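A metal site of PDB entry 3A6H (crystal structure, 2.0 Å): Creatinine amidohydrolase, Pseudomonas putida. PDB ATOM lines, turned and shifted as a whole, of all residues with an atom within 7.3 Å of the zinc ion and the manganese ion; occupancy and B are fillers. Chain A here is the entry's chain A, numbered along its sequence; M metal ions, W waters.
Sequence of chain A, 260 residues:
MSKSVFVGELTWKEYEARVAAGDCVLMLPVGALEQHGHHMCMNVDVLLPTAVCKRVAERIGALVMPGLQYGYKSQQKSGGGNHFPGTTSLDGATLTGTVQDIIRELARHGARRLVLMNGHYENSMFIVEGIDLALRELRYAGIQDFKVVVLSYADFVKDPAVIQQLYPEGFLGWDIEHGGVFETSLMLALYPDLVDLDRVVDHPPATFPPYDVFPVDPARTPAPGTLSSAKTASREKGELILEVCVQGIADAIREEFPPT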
ATOM      1  N   GLY A  31     -11.684  21.243  22.445  1.00  0.00           N
ATOM      2  CA  GLY A  31     -12.763  21.406  21.486  1.00  0.00           C
ATOM      3  C   GLY A  31     -13.986  20.531  21.656  1.00  0.00           C
ATOM      4  O   GLY A  31     -14.480  20.325  22.761  1.00  0.00           O
ATOM      5  N   ALA A  32     -14.472  20.011  20.529  1.00  0.00           N
ATOM      6  CA  ALA A  32     -15.655  19.178  20.516  1.00  0.00           C
ATOM      7  C   ALA A  32     -15.942  18.644  19.114  1.00  0.00           C
ATOM      8  O   ALA A  32     -15.381  19.134  18.134  1.00  0.00           O
ATOM      9  CB  ALA A  32     -16.856  19.986  20.989  1.00  0.00           C
ATOM     10  N   GLU A  34     -19.004  18.493  16.998  1.00  0.00           N
ATOM     11  CA  GLU A  34     -20.340  19.076  17.030  1.00  0.00           C
ATOM     12  C   GLU A  34     -20.788  19.580  15.669  1.00  0.00           C
ATOM     13  O   GLU A  34     -20.002  20.151  14.909  1.00  0.00           O
ATOM     14  CB  GLU A  34     -20.316  20.233  18.020  1.00  0.00           C
ATOM     15  CG  GLU A  34     -21.629  20.934  18.307  1.00  0.00           C
ATOM     16  CD  GLU A  34     -21.389  22.206  19.109  1.00  0.00           C
ATOM     17  OE1 GLU A  34     -22.214  22.564  19.983  1.00  0.00           O
ATOM     18  OE2 GLU A  34     -20.344  22.856  18.850  1.00  0.00           O
ATOM     19  N   GLN A  35     -22.077  19.401  15.373  1.00  0.00           N
ATOM     20  CA  GLN A  35     -22.630  19.849  14.109  1.00  0.00           C
ATOM     21  C   GLN A  35     -22.412  21.344  13.944  1.00  0.00           C
ATOM     22  O   GLN A  35     -22.573  22.120  14.895  1.00  0.00           O
ATOM     23  CB  GLN A  35     -24.123  19.522  14.022  1.00  0.00           C
ATOM     24  CG  GLN A  35     -25.052  20.299  14.966  1.00  0.00           C
ATOM     25  CD  GLN A  35     -25.316  21.731  14.514  1.00  0.00           C
ATOM     26  OE1 GLN A  35     -25.234  22.053  13.328  1.00  0.00           O
ATOM     27  NE2 GLN A  35     -25.667  22.597  15.467  1.00  0.00           N
ATOM     28  N   HIS A  36     -22.013  21.749  12.743  1.00  0.00           N
ATOM     29  CA  HIS A  36     -21.801  23.154  12.432  1.00  0.00           C
ATOM     30  C   HIS A  36     -22.516  23.519  11.120  1.00  0.00           C
ATOM     31  O   HIS A  36     -21.910  24.067  10.209  1.00  0.00           O
ATOM     32  CB  HIS A  36     -20.319  23.489  12.320  1.00  0.00           C
ATOM     33  CG  HIS A  36     -19.663  23.751  13.638  1.00  0.00           C
ATOM     34  ND1 HIS A  36     -19.370  22.749  14.546  1.00  0.00           N
ATOM     35  CD2 HIS A  36     -19.294  24.912  14.237  1.00  0.00           C
ATOM     36  CE1 HIS A  36     -18.841  23.289  15.633  1.00  0.00           C
ATOM     37  NE2 HIS A  36     -18.788  24.599  15.468  1.00  0.00           N
ATOM     38  N   MET A  40     -20.184  23.306   7.030  1.00  0.00           N
ATOM     39  CA  MET A  40     -18.878  23.041   7.635  1.00  0.00           C
ATOM     40  C   MET A  40     -18.787  21.664   8.275  1.00  0.00           C
ATOM     41  O   MET A  40     -19.801  21.068   8.646  1.00  0.00           O
ATOM     42  CB  MET A  40     -18.544  24.100   8.697  1.00  0.00           C
ATOM     43  CG  MET A  40     -18.392  25.499   8.192  1.00  0.00           C
ATOM     44  SD  MET A  40     -17.479  26.507   9.367  1.00  0.00           S
ATOM     45  CE  MET A  40     -18.746  26.964  10.542  1.00  0.00           C
ATOM     46  N   VAL A  44     -14.769  21.595  13.741  1.00  0.00           N
ATOM     47  CA  VAL A  44     -14.418  23.019  13.803  1.00  0.00           C
ATOM     48  C   VAL A  44     -13.896  23.480  15.181  1.00  0.00           C
ATOM     49  O   VAL A  44     -12.877  24.170  15.261  1.00  0.00           O
ATOM     50  CB  VAL A  44     -15.634  23.897  13.410  1.00  0.00           C
ATOM     51  CG1 VAL A  44     -15.372  25.372  13.729  1.00  0.00           C
ATOM     52  CG2 VAL A  44     -15.942  23.726  11.913  1.00  0.00           C
ATOM     53  N   ASP A  45     -14.589  23.105  16.253  1.00  0.00           N
ATOM     54  CA  ASP A  45     -14.176  23.498  17.607  1.00  0.00           C
ATOM     55  C   ASP A  45     -12.803  22.960  18.031  1.00  0.00           C
ATOM     56  O   ASP A  45     -12.239  23.433  19.011  1.00  0.00           O
ATOM     57  CB  ASP A  45     -15.227  23.084  18.631  1.00  0.00           C
ATOM     58  CG  ASP A  45     -16.494  23.909  18.523  1.00  0.00           C
ATOM     59  OD1 ASP A  45     -16.496  24.904  17.773  1.00  0.00           O
ATOM     60  OD2 ASP A  45     -17.491  23.569  19.189  1.00  0.00           O
ATOM     61  N   VAL A  46     -12.289  21.973  17.308  1.00  0.00           N
ATOM     62  CA  VAL A  46     -10.965  21.441  17.610  1.00  0.00           C
ATOM     63  C   VAL A  46      -9.958  22.115  16.683  1.00  0.00           C
ATOM     64  O   VAL A  46      -8.894  22.562  17.115  1.00  0.00           O
ATOM     65  CB  VAL A  46     -10.861  19.909  17.367  1.00  0.00           C
ATOM     66  CG1 VAL A  46      -9.400  19.471  17.479  1.00  0.00           C
ATOM     67  CG2 VAL A  46     -11.700  19.149  18.381  1.00  0.00           C
ATOM     68  N   LEU A  48     -10.056  25.065  14.960  1.00  0.00           N
ATOM     69  CA  LEU A  48      -9.785  26.478  15.188  1.00  0.00           C
ATOM     70  C   LEU A  48      -8.875  26.814  16.364  1.00  0.00           C
ATOM     71  O   LEU A  48      -7.883  27.509  16.194  1.00  0.00           O
ATOM     72  CB  LEU A  48     -11.101  27.257  15.258  1.00  0.00           C
ATOM     73  CG  LEU A  48     -11.911  27.162  13.955  1.00  0.00           C
ATOM     74  CD1 LEU A  48     -13.098  28.120  14.025  1.00  0.00           C
ATOM     75  CD2 LEU A  48     -11.025  27.507  12.744  1.00  0.00           C
ATOM     76  N   TYR A  72     -18.223  19.068  26.122  1.00  0.00           N
ATOM     77  CA  TYR A  72     -19.488  18.957  26.822  1.00  0.00           C
ATOM     78  C   TYR A  72     -20.711  19.075  25.897  1.00  0.00           C
ATOM     79  O   TYR A  72     -20.623  19.628  24.806  1.00  0.00           O
ATOM     80  CB  TYR A  72     -19.591  20.011  27.934  1.00  0.00           C
ATOM     81  CG  TYR A  72     -20.826  19.851  28.811  1.00  0.00           C
ATOM     82  CD1 TYR A  72     -20.998  18.713  29.605  1.00  0.00           C
ATOM     83  CD2 TYR A  72     -21.857  20.789  28.772  1.00  0.00           C
ATOM     84  CE1 TYR A  72     -22.169  18.506  30.337  1.00  0.00           C
ATOM     85  CE2 TYR A  72     -23.035  20.603  29.503  1.00  0.00           C
ATOM     86  CZ  TYR A  72     -23.189  19.457  30.275  1.00  0.00           C
ATOM     87  OH  TYR A  72     -24.367  19.240  30.965  1.00  0.00           O
ATOM     88  N   SER A  74     -23.713  19.896  23.719  1.00  0.00           N
ATOM     89  CA  SER A  74     -24.093  21.086  22.980  1.00  0.00           C
ATOM     90  C   SER A  74     -25.389  21.632  23.605  1.00  0.00           C
ATOM     91  O   SER A  74     -26.299  20.854  23.913  1.00  0.00           O
ATOM     92  CB  SER A  74     -24.334  20.711  21.505  1.00  0.00           C
ATOM     93  OG  SER A  74     -24.792  21.808  20.750  1.00  0.00           O
ATOM     94  N   SER A  78     -26.559  28.078  22.314  1.00  0.00           N
ATOM     95  CA  SER A  78     -25.163  28.349  22.008  1.00  0.00           C
ATOM     96  C   SER A  78     -24.627  27.476  20.874  1.00  0.00           C
ATOM     97  O   SER A  78     -23.880  27.956  20.021  1.00  0.00           O
ATOM     98  CB  SER A  78     -24.286  28.175  23.262  1.00  0.00           C
ATOM     99  OG  SER A  78     -24.453  26.892  23.832  1.00  0.00           O
ATOM    100  N   GLY A  79     -25.013  26.207  20.847  1.00  0.00           N
ATOM    101  CA  GLY A  79     -24.531  25.308  19.813  1.00  0.00           C
ATOM    102  C   GLY A  79     -25.618  24.563  19.044  1.00  0.00           C
ATOM    103  O   GLY A  79     -25.321  23.681  18.240  1.00  0.00           O
ATOM    104  N   GLY A 119     -12.535  26.162  22.579  1.00  0.00           N
ATOM    105  CA  GLY A 119     -13.110  26.495  21.286  1.00  0.00           C
ATOM    106  C   GLY A 119     -14.571  26.094  21.198  1.00  0.00           C
ATOM    107  O   GLY A 119     -15.193  26.244  20.146  1.00  0.00           O
ATOM    108  N   HIS A 120     -15.117  25.600  22.312  1.00  0.00           N
ATOM    109  CA  HIS A 120     -16.510  25.150  22.417  1.00  0.00           C
ATOM    110  C   HIS A 120     -17.090  25.757  23.706  1.00  0.00           C
ATOM    111  O   HIS A 120     -16.819  25.277  24.821  1.00  0.00           O
ATOM    112  CB  HIS A 120     -16.527  23.610  22.480  1.00  0.00           C
ATOM    113  CG  HIS A 120     -17.889  23.004  22.694  1.00  0.00           C
ATOM    114  ND1 HIS A 120     -18.934  23.188  21.822  1.00  0.00           N
ATOM    115  CD2 HIS A 120     -18.341  22.147  23.641  1.00  0.00           C
ATOM    116  CE1 HIS A 120     -19.975  22.482  22.225  1.00  0.00           C
ATOM    117  NE2 HIS A 120     -19.636  21.835  23.321  1.00  0.00           N
ATOM    118  N   TYR A 121     -17.900  26.801  23.554  1.00  0.00           N
ATOM    119  CA  TYR A 121     -18.505  27.526  24.673  1.00  0.00           C
ATOM    120  C   TYR A 121     -18.960  26.681  25.867  1.00  0.00           C
ATOM    121  O   TYR A 121     -18.606  26.973  27.010  1.00  0.00           O
ATOM    122  CB  TYR A 121     -19.680  28.368  24.165  1.00  0.00           C
ATOM    123  CG  TYR A 121     -20.232  29.290  25.215  1.00  0.00           C
ATOM    124  CD1 TYR A 121     -19.460  30.340  25.713  1.00  0.00           C
ATOM    125  CD2 TYR A 121     -21.508  29.102  25.748  1.00  0.00           C
ATOM    126  CE1 TYR A 121     -19.939  31.177  26.706  1.00  0.00           C
ATOM    127  CE2 TYR A 121     -22.001  29.938  26.743  1.00  0.00           C
ATOM    128  CZ  TYR A 121     -21.209  30.972  27.223  1.00  0.00           C
ATOM    129  OH  TYR A 121     -21.675  31.809  28.213  1.00  0.00           O
ATOM    130  N   GLU A 122     -19.733  25.643  25.591  1.00  0.00           N
ATOM    131  CA  GLU A 122     -20.253  24.758  26.641  1.00  0.00           C
ATOM    132  C   GLU A 122     -19.205  24.106  27.550  1.00  0.00           C
ATOM    133  O   GLU A 122     -19.547  23.661  28.651  1.00  0.00           O
ATOM    134  CB  GLU A 122     -21.132  23.666  26.004  1.00  0.00           C
ATOM    135  CG  GLU A 122     -22.430  24.197  25.376  1.00  0.00           C
ATOM    136  CD  GLU A 122     -22.258  24.685  23.949  1.00  0.00           C
ATOM    137  OE1 GLU A 122     -21.179  25.226  23.610  1.00  0.00           O
ATOM    138  OE2 GLU A 122     -23.218  24.545  23.169  1.00  0.00           O
ATOM    139  N   ASN A 123     -17.956  24.056  27.109  1.00  0.00           N
ATOM    140  CA  ASN A 123     -16.878  23.446  27.908  1.00  0.00           C
ATOM    141  C   ASN A 123     -16.454  24.261  29.119  1.00  0.00           C
ATOM    142  O   ASN A 123     -16.012  23.704  30.119  1.00  0.00           O
ATOM    143  CB  ASN A 123     -15.609  23.241  27.072  1.00  0.00           C
ATOM    144  CG  ASN A 123     -15.740  22.175  26.015  1.00  0.00           C
ATOM    145  OD1 ASN A 123     -16.498  21.220  26.163  1.00  0.00           O
ATOM    146  ND2 ASN A 123     -14.974  22.315  24.941  1.00  0.00           N
ATOM    147  N   TYR A 153     -10.570  32.040  22.359  1.00  0.00           N
ATOM    148  CA  TYR A 153      -9.946  32.910  21.373  1.00  0.00           C
ATOM    149  C   TYR A 153     -10.832  34.026  20.813  1.00  0.00           C
ATOM    150  O   TYR A 153     -10.350  35.129  20.549  1.00  0.00           O
ATOM    151  CB  TYR A 153      -9.346  32.067  20.240  1.00  0.00           C
ATOM    152  CG  TYR A 153     -10.352  31.396  19.322  1.00  0.00           C
ATOM    153  CD1 TYR A 153     -10.910  32.089  18.259  1.00  0.00           C
ATOM    154  CD2 TYR A 153     -10.754  30.073  19.543  1.00  0.00           C
ATOM    155  CE1 TYR A 153     -11.841  31.483  17.418  1.00  0.00           C
ATOM    156  CE2 TYR A 153     -11.691  29.470  18.710  1.00  0.00           C
ATOM    157  CZ  TYR A 153     -12.228  30.175  17.646  1.00  0.00           C
ATOM    158  OH  TYR A 153     -13.171  29.599  16.824  1.00  0.00           O
ATOM    159  N   GLU A 177     -23.605  33.354  17.058  1.00  0.00           N
ATOM    160  CA  GLU A 177     -22.530  33.014  16.140  1.00  0.00           C
ATOM    161  C   GLU A 177     -22.265  31.559  15.759  1.00  0.00           C
ATOM    162  O   GLU A 177     -21.505  31.316  14.818  1.00  0.00           O
ATOM    163  CB  GLU A 177     -21.224  33.671  16.611  1.00  0.00           C
ATOM    164  CG  GLU A 177     -21.064  35.097  16.116  1.00  0.00           C
ATOM    165  CD  GLU A 177     -20.954  35.189  14.609  1.00  0.00           C
ATOM    166  OE1 GLU A 177     -21.337  36.235  14.040  1.00  0.00           O
ATOM    167  OE2 GLU A 177     -20.476  34.215  13.972  1.00  0.00           O
ATOM    168  N   HIS A 178     -22.863  30.588  16.443  1.00  0.00           N
ATOM    169  CA  HIS A 178     -22.593  29.183  16.101  1.00  0.00           C
ATOM    170  C   HIS A 178     -22.776  28.893  14.602  1.00  0.00           C
ATOM    171  O   HIS A 178     -23.896  28.950  14.076  1.00  0.00           O
ATOM    172  CB  HIS A 178     -23.487  28.246  16.906  1.00  0.00           C
ATOM    173  CG  HIS A 178     -23.233  26.795  16.636  1.00  0.00           C
ATOM    174  ND1 HIS A 178     -22.033  26.180  16.907  1.00  0.00           N
ATOM    175  CD2 HIS A 178     -24.024  25.832  16.091  1.00  0.00           C
ATOM    176  CE1 HIS A 178     -22.086  24.909  16.550  1.00  0.00           C
ATOM    177  NE2 HIS A 178     -23.283  24.673  16.054  1.00  0.00           N
ATOM    178  N   GLY A 179     -21.667  28.560  13.935  1.00  0.00           N
ATOM    179  CA  GLY A 179     -21.694  28.266  12.510  1.00  0.00           C
ATOM    180  C   GLY A 179     -21.985  29.496  11.668  1.00  0.00           C
ATOM    181  O   GLY A 179     -22.345  29.398  10.491  1.00  0.00           O
ATOM    182  N   GLU A 183     -16.834  31.926  12.870  1.00  0.00           N
ATOM    183  CA  GLU A 183     -16.121  30.665  12.688  1.00  0.00           C
ATOM    184  C   GLU A 183     -15.971  30.299  11.231  1.00  0.00           C
ATOM    185  O   GLU A 183     -14.948  29.746  10.830  1.00  0.00           O
ATOM    186  CB  GLU A 183     -16.849  29.500  13.363  1.00  0.00           C
ATOM    187  CG  GLU A 183     -17.225  29.687  14.795  1.00  0.00           C
ATOM    188  CD  GLU A 183     -17.871  28.438  15.340  1.00  0.00           C
ATOM    189  OE1 GLU A 183     -17.153  27.624  15.948  1.00  0.00           O
ATOM    190  OE2 GLU A 183     -19.090  28.246  15.118  1.00  0.00           O
HETATM  191 ZN    ZN M   1     -18.239  26.094  17.028  1.00  0.00          ZN
HETATM  192 MN    MN M   2     -19.288  24.557  20.010  1.00  0.00          MN
HETATM  193  O   HOH W   1     -21.269  25.193  20.756  1.00  0.00           O
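The side-chain amide nitrogen (ND2) of Asn 123 lies close to the backbone carbonyl oxygen (O) of His 120, at 3.5 Å.
NE2 of His 178 lies within hydrogen-bond range of O of Gln 35, 2.9 Å away.
A ring nitrogen (NE2) of His 178 sits at hydrogen-bond distance from the backbone carbonyl oxygen (O) of Gly 79, 3.1 Å away.
NE2 of His 120 sits at hydrogen-bond distance from O of Tyr 72.
ND1 of His 36 is in hydrogen-bond range of O of Glu 34 (2.7 Å).
N of Gly 179 is in hydrogen-bond range of OE2 of Glu 183 (2.9 Å).
The side-chain hydroxyl of Ser 74 sits at hydrogen-bond distance from the side-chain carboxylate of Glu 34 (2.8 Å).
Merely in contact with the zinc ion: His 178 (3.8 Å).
The nearest printed residue that does not touch the zinc ion is Glu 34 (4.3 Å).
Of the 24 residues printed, 3 come within 4 Å of the manganese ion.
The nearest printed residue that does not touch the manganese ion is Glu 122 (4.1 Å).
The zinc ion is bound by OE1 of Glu 183, NE2 of His 36 and OD1 of Asp 45.
The zinc ion has three donor atoms within binding distance.
The manganese ion is bound by OD2 of Asp 45 (2.2 Å).
Water W1 is bound to the manganese ion (2.2 Å).
The manganese ion is bound by ND1 of His 120 (2.3 Å).
OE2 of Glu 34 binds the manganese ion, at 2.3 Å.
The manganese ion has four donor atoms within binding distance.
Water W1 lies within hydrogen-bond range of OE1 of Glu 122 and OE1 of Glu 34.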
